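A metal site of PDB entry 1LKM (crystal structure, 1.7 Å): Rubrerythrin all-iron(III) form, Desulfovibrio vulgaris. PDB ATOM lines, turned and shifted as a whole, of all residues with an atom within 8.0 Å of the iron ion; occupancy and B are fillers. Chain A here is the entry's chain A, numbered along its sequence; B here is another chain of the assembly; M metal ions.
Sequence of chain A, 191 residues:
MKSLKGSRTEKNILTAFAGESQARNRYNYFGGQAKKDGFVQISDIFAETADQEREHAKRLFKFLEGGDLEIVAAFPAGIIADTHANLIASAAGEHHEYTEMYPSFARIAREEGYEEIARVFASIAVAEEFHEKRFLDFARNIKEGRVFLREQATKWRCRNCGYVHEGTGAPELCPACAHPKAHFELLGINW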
ATOM      1  N   ARG A 157     -24.662 -11.963 -13.772  1.00  0.00           N
ATOM      2  CA  ARG A 157     -24.952 -10.572 -13.448  1.00  0.00           C
ATOM      3  C   ARG A 157     -25.084  -9.737 -14.709  1.00  0.00           C
ATOM      4  O   ARG A 157     -24.309  -9.887 -15.648  1.00  0.00           O
ATOM      5  CB  ARG A 157     -23.839  -9.979 -12.580  1.00  0.00           C
ATOM      6  CG  ARG A 157     -24.169  -8.580 -12.042  1.00  0.00           C
ATOM      7  CD  ARG A 157     -22.996  -7.949 -11.303  1.00  0.00           C
ATOM      8  NE  ARG A 157     -21.926  -7.542 -12.214  1.00  0.00           N
ATOM      9  CZ  ARG A 157     -21.476  -6.299 -12.345  1.00  0.00           C
ATOM     10  NH1 ARG A 157     -21.993  -5.324 -11.617  1.00  0.00           N
ATOM     11  NH2 ARG A 157     -20.500  -6.033 -13.209  1.00  0.00           N
ATOM     12  N   CYS A 158     -26.086  -8.848 -14.726  1.00  0.00           N
ATOM     13  CA  CYS A 158     -26.284  -7.958 -15.850  1.00  0.00           C
ATOM     14  C   CYS A 158     -25.317  -6.791 -15.639  1.00  0.00           C
ATOM     15  O   CYS A 158     -25.375  -6.116 -14.618  1.00  0.00           O
ATOM     16  CB  CYS A 158     -27.724  -7.434 -15.875  1.00  0.00           C
ATOM     17  SG  CYS A 158     -27.995  -6.192 -17.159  1.00  0.00           S
ATOM     18  N   ARG A 159     -24.412  -6.566 -16.592  1.00  0.00           N
ATOM     19  CA  ARG A 159     -23.463  -5.471 -16.451  1.00  0.00           C
ATOM     20  C   ARG A 159     -24.127  -4.109 -16.583  1.00  0.00           C
ATOM     21  O   ARG A 159     -23.618  -3.110 -16.065  1.00  0.00           O
ATOM     22  CB  ARG A 159     -22.342  -5.602 -17.489  1.00  0.00           C
ATOM     23  CG  ARG A 159     -21.370  -6.748 -17.226  1.00  0.00           C
ATOM     24  CD  ARG A 159     -20.266  -6.802 -18.266  1.00  0.00           C
ATOM     25  NE  ARG A 159     -19.445  -5.591 -18.272  1.00  0.00           N
ATOM     26  CZ  ARG A 159     -18.561  -5.274 -17.338  1.00  0.00           C
ATOM     27  NH1 ARG A 159     -18.349  -6.075 -16.305  1.00  0.00           N
ATOM     28  NH2 ARG A 159     -17.879  -4.130 -17.433  1.00  0.00           N
ATOM     29  N   ASN A 160     -25.285  -4.066 -17.244  1.00  0.00           N
ATOM     30  CA  ASN A 160     -25.979  -2.804 -17.434  1.00  0.00           C
ATOM     31  C   ASN A 160     -26.690  -2.273 -16.187  1.00  0.00           C
ATOM     32  O   ASN A 160     -26.613  -1.067 -15.902  1.00  0.00           O
ATOM     33  CB  ASN A 160     -27.014  -2.945 -18.574  1.00  0.00           C
ATOM     34  CG  ASN A 160     -27.621  -1.608 -18.980  1.00  0.00           C
ATOM     35  OD1 ASN A 160     -28.829  -1.406 -18.895  1.00  0.00           O
ATOM     36  ND2 ASN A 160     -26.767  -0.692 -19.425  1.00  0.00           N
ATOM     37  N   CYS A 161     -27.349  -3.148 -15.429  1.00  0.00           N
ATOM     38  CA  CYS A 161     -28.090  -2.709 -14.245  1.00  0.00           C
ATOM     39  C   CYS A 161     -27.779  -3.425 -12.932  1.00  0.00           C
ATOM     40  O   CYS A 161     -28.247  -2.987 -11.874  1.00  0.00           O
ATOM     41  CB  CYS A 161     -29.591  -2.804 -14.513  1.00  0.00           C
ATOM     42  SG  CYS A 161     -30.259  -4.483 -14.473  1.00  0.00           S
ATOM     43  N   GLY A 162     -27.035  -4.521 -12.993  1.00  0.00           N
ATOM     44  CA  GLY A 162     -26.690  -5.239 -11.777  1.00  0.00           C
ATOM     45  C   GLY A 162     -27.620  -6.382 -11.407  1.00  0.00           C
ATOM     46  O   GLY A 162     -27.429  -7.027 -10.376  1.00  0.00           O
ATOM     47  N   TYR A 163     -28.633  -6.637 -12.227  1.00  0.00           N
ATOM     48  CA  TYR A 163     -29.546  -7.735 -11.925  1.00  0.00           C
ATOM     49  C   TYR A 163     -28.787  -9.054 -11.854  1.00  0.00           C
ATOM     50  O   TYR A 163     -27.862  -9.287 -12.627  1.00  0.00           O
ATOM     51  CB  TYR A 163     -30.629  -7.837 -13.005  1.00  0.00           C
ATOM     52  CG  TYR A 163     -31.594  -8.981 -12.761  1.00  0.00           C
ATOM     53  CD1 TYR A 163     -32.560  -8.896 -11.768  1.00  0.00           C
ATOM     54  CD2 TYR A 163     -31.500 -10.163 -13.501  1.00  0.00           C
ATOM     55  CE1 TYR A 163     -33.415  -9.973 -11.499  1.00  0.00           C
ATOM     56  CE2 TYR A 163     -32.340 -11.235 -13.247  1.00  0.00           C
ATOM     57  CZ  TYR A 163     -33.295 -11.133 -12.245  1.00  0.00           C
ATOM     58  OH  TYR A 163     -34.143 -12.194 -11.990  1.00  0.00           O
ATOM     59  N   VAL A 164     -29.176  -9.910 -10.904  1.00  0.00           N
ATOM     60  CA  VAL A 164     -28.538 -11.214 -10.742  1.00  0.00           C
ATOM     61  C   VAL A 164     -29.532 -12.309 -11.116  1.00  0.00           C
ATOM     62  O   VAL A 164     -30.627 -12.376 -10.568  1.00  0.00           O
ATOM     63  CB  VAL A 164     -28.050 -11.429  -9.297  1.00  0.00           C
ATOM     64  CG1 VAL A 164     -27.469 -12.832  -9.144  1.00  0.00           C
ATOM     65  CG2 VAL A 164     -27.005 -10.383  -8.938  1.00  0.00           C
ATOM     66  N   LEU A 173     -33.286 -11.751 -22.130  1.00  0.00           N
ATOM     67  CA  LEU A 173     -33.514 -10.348 -21.793  1.00  0.00           C
ATOM     68  C   LEU A 173     -33.432 -10.166 -20.286  1.00  0.00           C
ATOM     69  O   LEU A 173     -33.918 -10.993 -19.529  1.00  0.00           O
ATOM     70  CB  LEU A 173     -34.906  -9.898 -22.269  1.00  0.00           C
ATOM     71  CG  LEU A 173     -35.168  -9.763 -23.769  1.00  0.00           C
ATOM     72  CD1 LEU A 173     -36.635  -9.400 -23.990  1.00  0.00           C
ATOM     73  CD2 LEU A 173     -34.260  -8.702 -24.358  1.00  0.00           C
ATOM     74  N   CYS A 174     -32.796  -9.078 -19.854  1.00  0.00           N
ATOM     75  CA  CYS A 174     -32.702  -8.818 -18.418  1.00  0.00           C
ATOM     76  C   CYS A 174     -34.094  -8.428 -17.948  1.00  0.00           C
ATOM     77  O   CYS A 174     -34.709  -7.512 -18.487  1.00  0.00           O
ATOM     78  CB  CYS A 174     -31.733  -7.664 -18.143  1.00  0.00           C
ATOM     79  SG  CYS A 174     -31.650  -7.227 -16.389  1.00  0.00           S
ATOM     80  N   PRO A 175     -34.627  -9.132 -16.924  1.00  0.00           N
ATOM     81  CA  PRO A 175     -35.958  -8.785 -16.437  1.00  0.00           C
ATOM     82  C   PRO A 175     -36.054  -7.418 -15.775  1.00  0.00           C
ATOM     83  O   PRO A 175     -37.136  -6.867 -15.627  1.00  0.00           O
ATOM     84  CB  PRO A 175     -36.281  -9.932 -15.471  1.00  0.00           C
ATOM     85  CG  PRO A 175     -34.951 -10.325 -14.962  1.00  0.00           C
ATOM     86  CD  PRO A 175     -34.080 -10.295 -16.200  1.00  0.00           C
ATOM     87  N   ALA A 176     -34.911  -6.856 -15.384  1.00  0.00           N
ATOM     88  CA  ALA A 176     -34.903  -5.541 -14.750  1.00  0.00           C
ATOM     89  C   ALA A 176     -34.777  -4.393 -15.752  1.00  0.00           C
ATOM     90  O   ALA A 176     -35.641  -3.528 -15.813  1.00  0.00           O
ATOM     91  CB  ALA A 176     -33.770  -5.458 -13.715  1.00  0.00           C
ATOM     92  N   CYS A 177     -33.714  -4.396 -16.560  1.00  0.00           N
ATOM     93  CA  CYS A 177     -33.492  -3.310 -17.522  1.00  0.00           C
ATOM     94  C   CYS A 177     -33.835  -3.613 -18.982  1.00  0.00           C
ATOM     95  O   CYS A 177     -33.650  -2.753 -19.852  1.00  0.00           O
ATOM     96  CB  CYS A 177     -32.042  -2.826 -17.453  1.00  0.00           C
ATOM     97  SG  CYS A 177     -30.857  -3.978 -18.161  1.00  0.00           S
ATOM     98  N   ALA A 178     -34.332  -4.818 -19.249  1.00  0.00           N
ATOM     99  CA  ALA A 178     -34.725  -5.222 -20.594  1.00  0.00           C
ATOM    100  C   ALA A 178     -33.610  -5.259 -21.625  1.00  0.00           C
ATOM    101  O   ALA A 178     -33.870  -5.341 -22.828  1.00  0.00           O
ATOM    102  CB  ALA A 178     -35.864  -4.336 -21.094  1.00  0.00           C
ATOM    103  N   HIS A 179     -32.357  -5.192 -21.179  1.00  0.00           N
ATOM    104  CA  HIS A 179     -31.246  -5.265 -22.128  1.00  0.00           C
ATOM    105  C   HIS A 179     -31.007  -6.720 -22.501  1.00  0.00           C
ATOM    106  O   HIS A 179     -31.338  -7.634 -21.736  1.00  0.00           O
ATOM    107  CB  HIS A 179     -29.993  -4.612 -21.554  1.00  0.00           C
ATOM    108  CG  HIS A 179     -29.968  -3.127 -21.702  1.00  0.00           C
ATOM    109  ND1 HIS A 179     -30.974  -2.314 -21.215  1.00  0.00           N
ATOM    110  CD2 HIS A 179     -29.094  -2.307 -22.336  1.00  0.00           C
ATOM    111  CE1 HIS A 179     -30.717  -1.066 -21.545  1.00  0.00           C
ATOM    112  NE2 HIS A 179     -29.581  -1.029 -22.223  1.00  0.00           N
ATOM    113  N   PRO A 180     -30.455  -6.965 -23.698  1.00  0.00           N
ATOM    114  CA  PRO A 180     -30.182  -8.322 -24.171  1.00  0.00           C
ATOM    115  C   PRO A 180     -29.128  -9.114 -23.414  1.00  0.00           C
ATOM    116  O   PRO A 180     -28.303  -8.558 -22.685  1.00  0.00           O
ATOM    117  CB  PRO A 180     -29.805  -8.108 -25.634  1.00  0.00           C
ATOM    118  CG  PRO A 180     -29.116  -6.797 -25.603  1.00  0.00           C
ATOM    119  CD  PRO A 180     -30.028  -5.975 -24.701  1.00  0.00           C
ATOM    120  N   HIS A 183     -25.313  -8.476 -22.306  1.00  0.00           N
ATOM    121  CA  HIS A 183     -24.811  -7.746 -21.154  1.00  0.00           C
ATOM    122  C   HIS A 183     -24.450  -8.596 -19.931  1.00  0.00           C
ATOM    123  O   HIS A 183     -23.860  -8.088 -18.980  1.00  0.00           O
ATOM    124  CB  HIS A 183     -25.823  -6.670 -20.745  1.00  0.00           C
ATOM    125  CG  HIS A 183     -25.948  -5.567 -21.755  1.00  0.00           C
ATOM    126  ND1 HIS A 183     -25.236  -4.387 -21.654  1.00  0.00           N
ATOM    127  CD2 HIS A 183     -26.651  -5.490 -22.913  1.00  0.00           C
ATOM    128  CE1 HIS A 183     -25.495  -3.639 -22.717  1.00  0.00           C
ATOM    129  NE2 HIS A 183     -26.346  -4.285 -23.485  1.00  0.00           N
ATOM    130  N   PHE A 184     -24.791  -9.877 -19.954  1.00  0.00           N
ATOM    131  CA  PHE A 184     -24.512 -10.740 -18.812  1.00  0.00           C
ATOM    132  C   PHE A 184     -23.123 -11.363 -18.730  1.00  0.00           C
ATOM    133  O   PHE A 184     -22.470 -11.622 -19.732  1.00  0.00           O
ATOM    134  CB  PHE A 184     -25.555 -11.862 -18.731  1.00  0.00           C
ATOM    135  CG  PHE A 184     -26.902 -11.401 -18.240  1.00  0.00           C
ATOM    136  CD1 PHE A 184     -27.833 -10.864 -19.135  1.00  0.00           C
ATOM    137  CD2 PHE A 184     -27.227 -11.476 -16.887  1.00  0.00           C
ATOM    138  CE1 PHE A 184     -29.076 -10.409 -18.670  1.00  0.00           C
ATOM    139  CE2 PHE A 184     -28.461 -11.032 -16.423  1.00  0.00           C
ATOM    140  CZ  PHE A 184     -29.392 -10.495 -17.318  1.00  0.00           C
ATOM    141  N   GLN B  52     -25.471   1.997 -13.014  1.00  0.00           N
ATOM    142  CA  GLN B  52     -26.554   1.020 -12.997  1.00  0.00           C
ATOM    143  C   GLN B  52     -27.826   1.681 -12.458  1.00  0.00           C
ATOM    144  O   GLN B  52     -28.921   1.343 -12.906  1.00  0.00           O
ATOM    145  CB  GLN B  52     -26.134  -0.224 -12.191  1.00  0.00           C
ATOM    146  CG  GLN B  52     -24.868  -0.849 -12.790  1.00  0.00           C
ATOM    147  CD  GLN B  52     -24.477  -2.181 -12.193  1.00  0.00           C
ATOM    148  OE1 GLN B  52     -24.641  -2.416 -10.995  1.00  0.00           O
ATOM    149  NE2 GLN B  52     -23.931  -3.071 -13.023  1.00  0.00           N
ATOM    150  N   GLU B  55     -29.544   3.281 -15.188  1.00  0.00           N
ATOM    151  CA  GLU B  55     -30.316   2.348 -15.997  1.00  0.00           C
ATOM    152  C   GLU B  55     -31.637   1.932 -15.328  1.00  0.00           C
ATOM    153  O   GLU B  55     -32.648   1.759 -16.013  1.00  0.00           O
ATOM    154  CB  GLU B  55     -29.459   1.128 -16.336  1.00  0.00           C
ATOM    155  CG  GLU B  55     -28.237   1.489 -17.204  1.00  0.00           C
ATOM    156  CD  GLU B  55     -28.644   2.156 -18.510  1.00  0.00           C
ATOM    157  OE1 GLU B  55     -29.524   1.607 -19.196  1.00  0.00           O
ATOM    158  OE2 GLU B  55     -28.078   3.207 -18.852  1.00  0.00           O
ATOM    159  N   HIS B  56     -31.644   1.768 -14.017  1.00  0.00           N
ATOM    160  CA  HIS B  56     -32.892   1.435 -13.329  1.00  0.00           C
ATOM    161  C   HIS B  56     -33.832   2.621 -13.542  1.00  0.00           C
ATOM    162  O   HIS B  56     -35.025   2.456 -13.839  1.00  0.00           O
ATOM    163  CB  HIS B  56     -32.653   1.254 -11.826  1.00  0.00           C
ATOM    164  CG  HIS B  56     -31.919  -0.005 -11.485  1.00  0.00           C
ATOM    165  ND1 HIS B  56     -31.156  -0.134 -10.347  1.00  0.00           N
ATOM    166  CD2 HIS B  56     -31.828  -1.187 -12.137  1.00  0.00           C
ATOM    167  CE1 HIS B  56     -30.616  -1.344 -10.316  1.00  0.00           C
ATOM    168  NE2 HIS B  56     -31.007  -2.001 -11.388  1.00  0.00           N
ATOM    169  N   ARG B  59     -35.368   2.693 -17.125  1.00  0.00           N
ATOM    170  CA  ARG B  59     -36.455   1.735 -17.288  1.00  0.00           C
ATOM    171  C   ARG B  59     -37.724   2.312 -16.673  1.00  0.00           C
ATOM    172  O   ARG B  59     -38.810   2.234 -17.251  1.00  0.00           O
ATOM    173  CB  ARG B  59     -36.108   0.397 -16.608  1.00  0.00           C
ATOM    174  CG  ARG B  59     -37.144  -0.713 -16.853  1.00  0.00           C
ATOM    175  CD  ARG B  59     -37.181  -1.106 -18.316  1.00  0.00           C
ATOM    176  NE  ARG B  59     -38.343  -1.919 -18.687  1.00  0.00           N
ATOM    177  CZ  ARG B  59     -38.473  -3.222 -18.458  1.00  0.00           C
ATOM    178  NH1 ARG B  59     -37.506  -3.891 -17.843  1.00  0.00           N
ATOM    179  NH2 ARG B  59     -39.561  -3.865 -18.862  1.00  0.00           N
ATOM    180  N   SER B 123     -37.687  -7.098  -9.952  1.00  0.00           N
ATOM    181  CA  SER B 123     -36.414  -7.446 -10.562  1.00  0.00           C
ATOM    182  C   SER B 123     -35.331  -6.445 -10.164  1.00  0.00           C
ATOM    183  O   SER B 123     -34.198  -6.833  -9.879  1.00  0.00           O
ATOM    184  CB  SER B 123     -36.555  -7.503 -12.078  1.00  0.00           C
ATOM    185  OG  SER B 123     -37.400  -8.578 -12.458  1.00  0.00           O
ATOM    186  N   ALA B 127     -31.214  -6.547  -8.005  1.00  0.00           N
ATOM    187  CA  ALA B 127     -29.960  -5.858  -8.293  1.00  0.00           C
ATOM    188  C   ALA B 127     -29.519  -5.054  -7.078  1.00  0.00           C
ATOM    189  O   ALA B 127     -28.334  -5.025  -6.738  1.00  0.00           O
ATOM    190  CB  ALA B 127     -30.125  -4.936  -9.492  1.00  0.00           C
HETATM  191 FE    FE M   1     -30.138  -5.442 -16.520  1.00  0.00          FE
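The backbone NH (N) of Asn 160 lies close to the side-chain sulfur (SG) of Cys 158, at 3.4 Å. The backbone NH (N) of Cys 158 is in hydrogen-bond range of the backbone carbonyl oxygen (O) of Tyr 163. NE2 of His 56 of chain B is in hydrogen-bond range of O of Cys 161, 3.0 Å away. The side-chain sulfur (SG) of Cys 174 lies close to the backbone NH (N) of Ala 176 (3.4 Å). The backbone NH of Tyr 163 sits close to the side-chain sulfur of Cys 161 (3.5 Å). N of Cys 174 is in hydrogen-bond range of O of His 179, at 2.8 Å. The side-chain amide oxygen (OD1) of Asn 160 lies close to the side-chain sulfur (SG) of Cys 177, 3.4 Å away. The backbone carbonyl oxygen of Cys 177 is in hydrogen-bond range of a ring nitrogen (ND1) of His 179, at 3.0 Å.
Four residues have an atom within 4 Å of the iron ion: Cys 158, Cys 161, Cys 174 and Cys 177. Along chain A the residues within 4 Å of the iron ion span positions 158 to 177.
The iron ion is bound by SG of Cys 161, at 2.3 Å. The side-chain sulfur (SG) of Cys 177 is bound to the iron ion, 2.3 Å away. The side-chain sulfur (SG) of Cys 174 binds the iron ion (2.3 Å). The side-chain sulfur (SG) of Cys 158 is bound to the iron ion.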
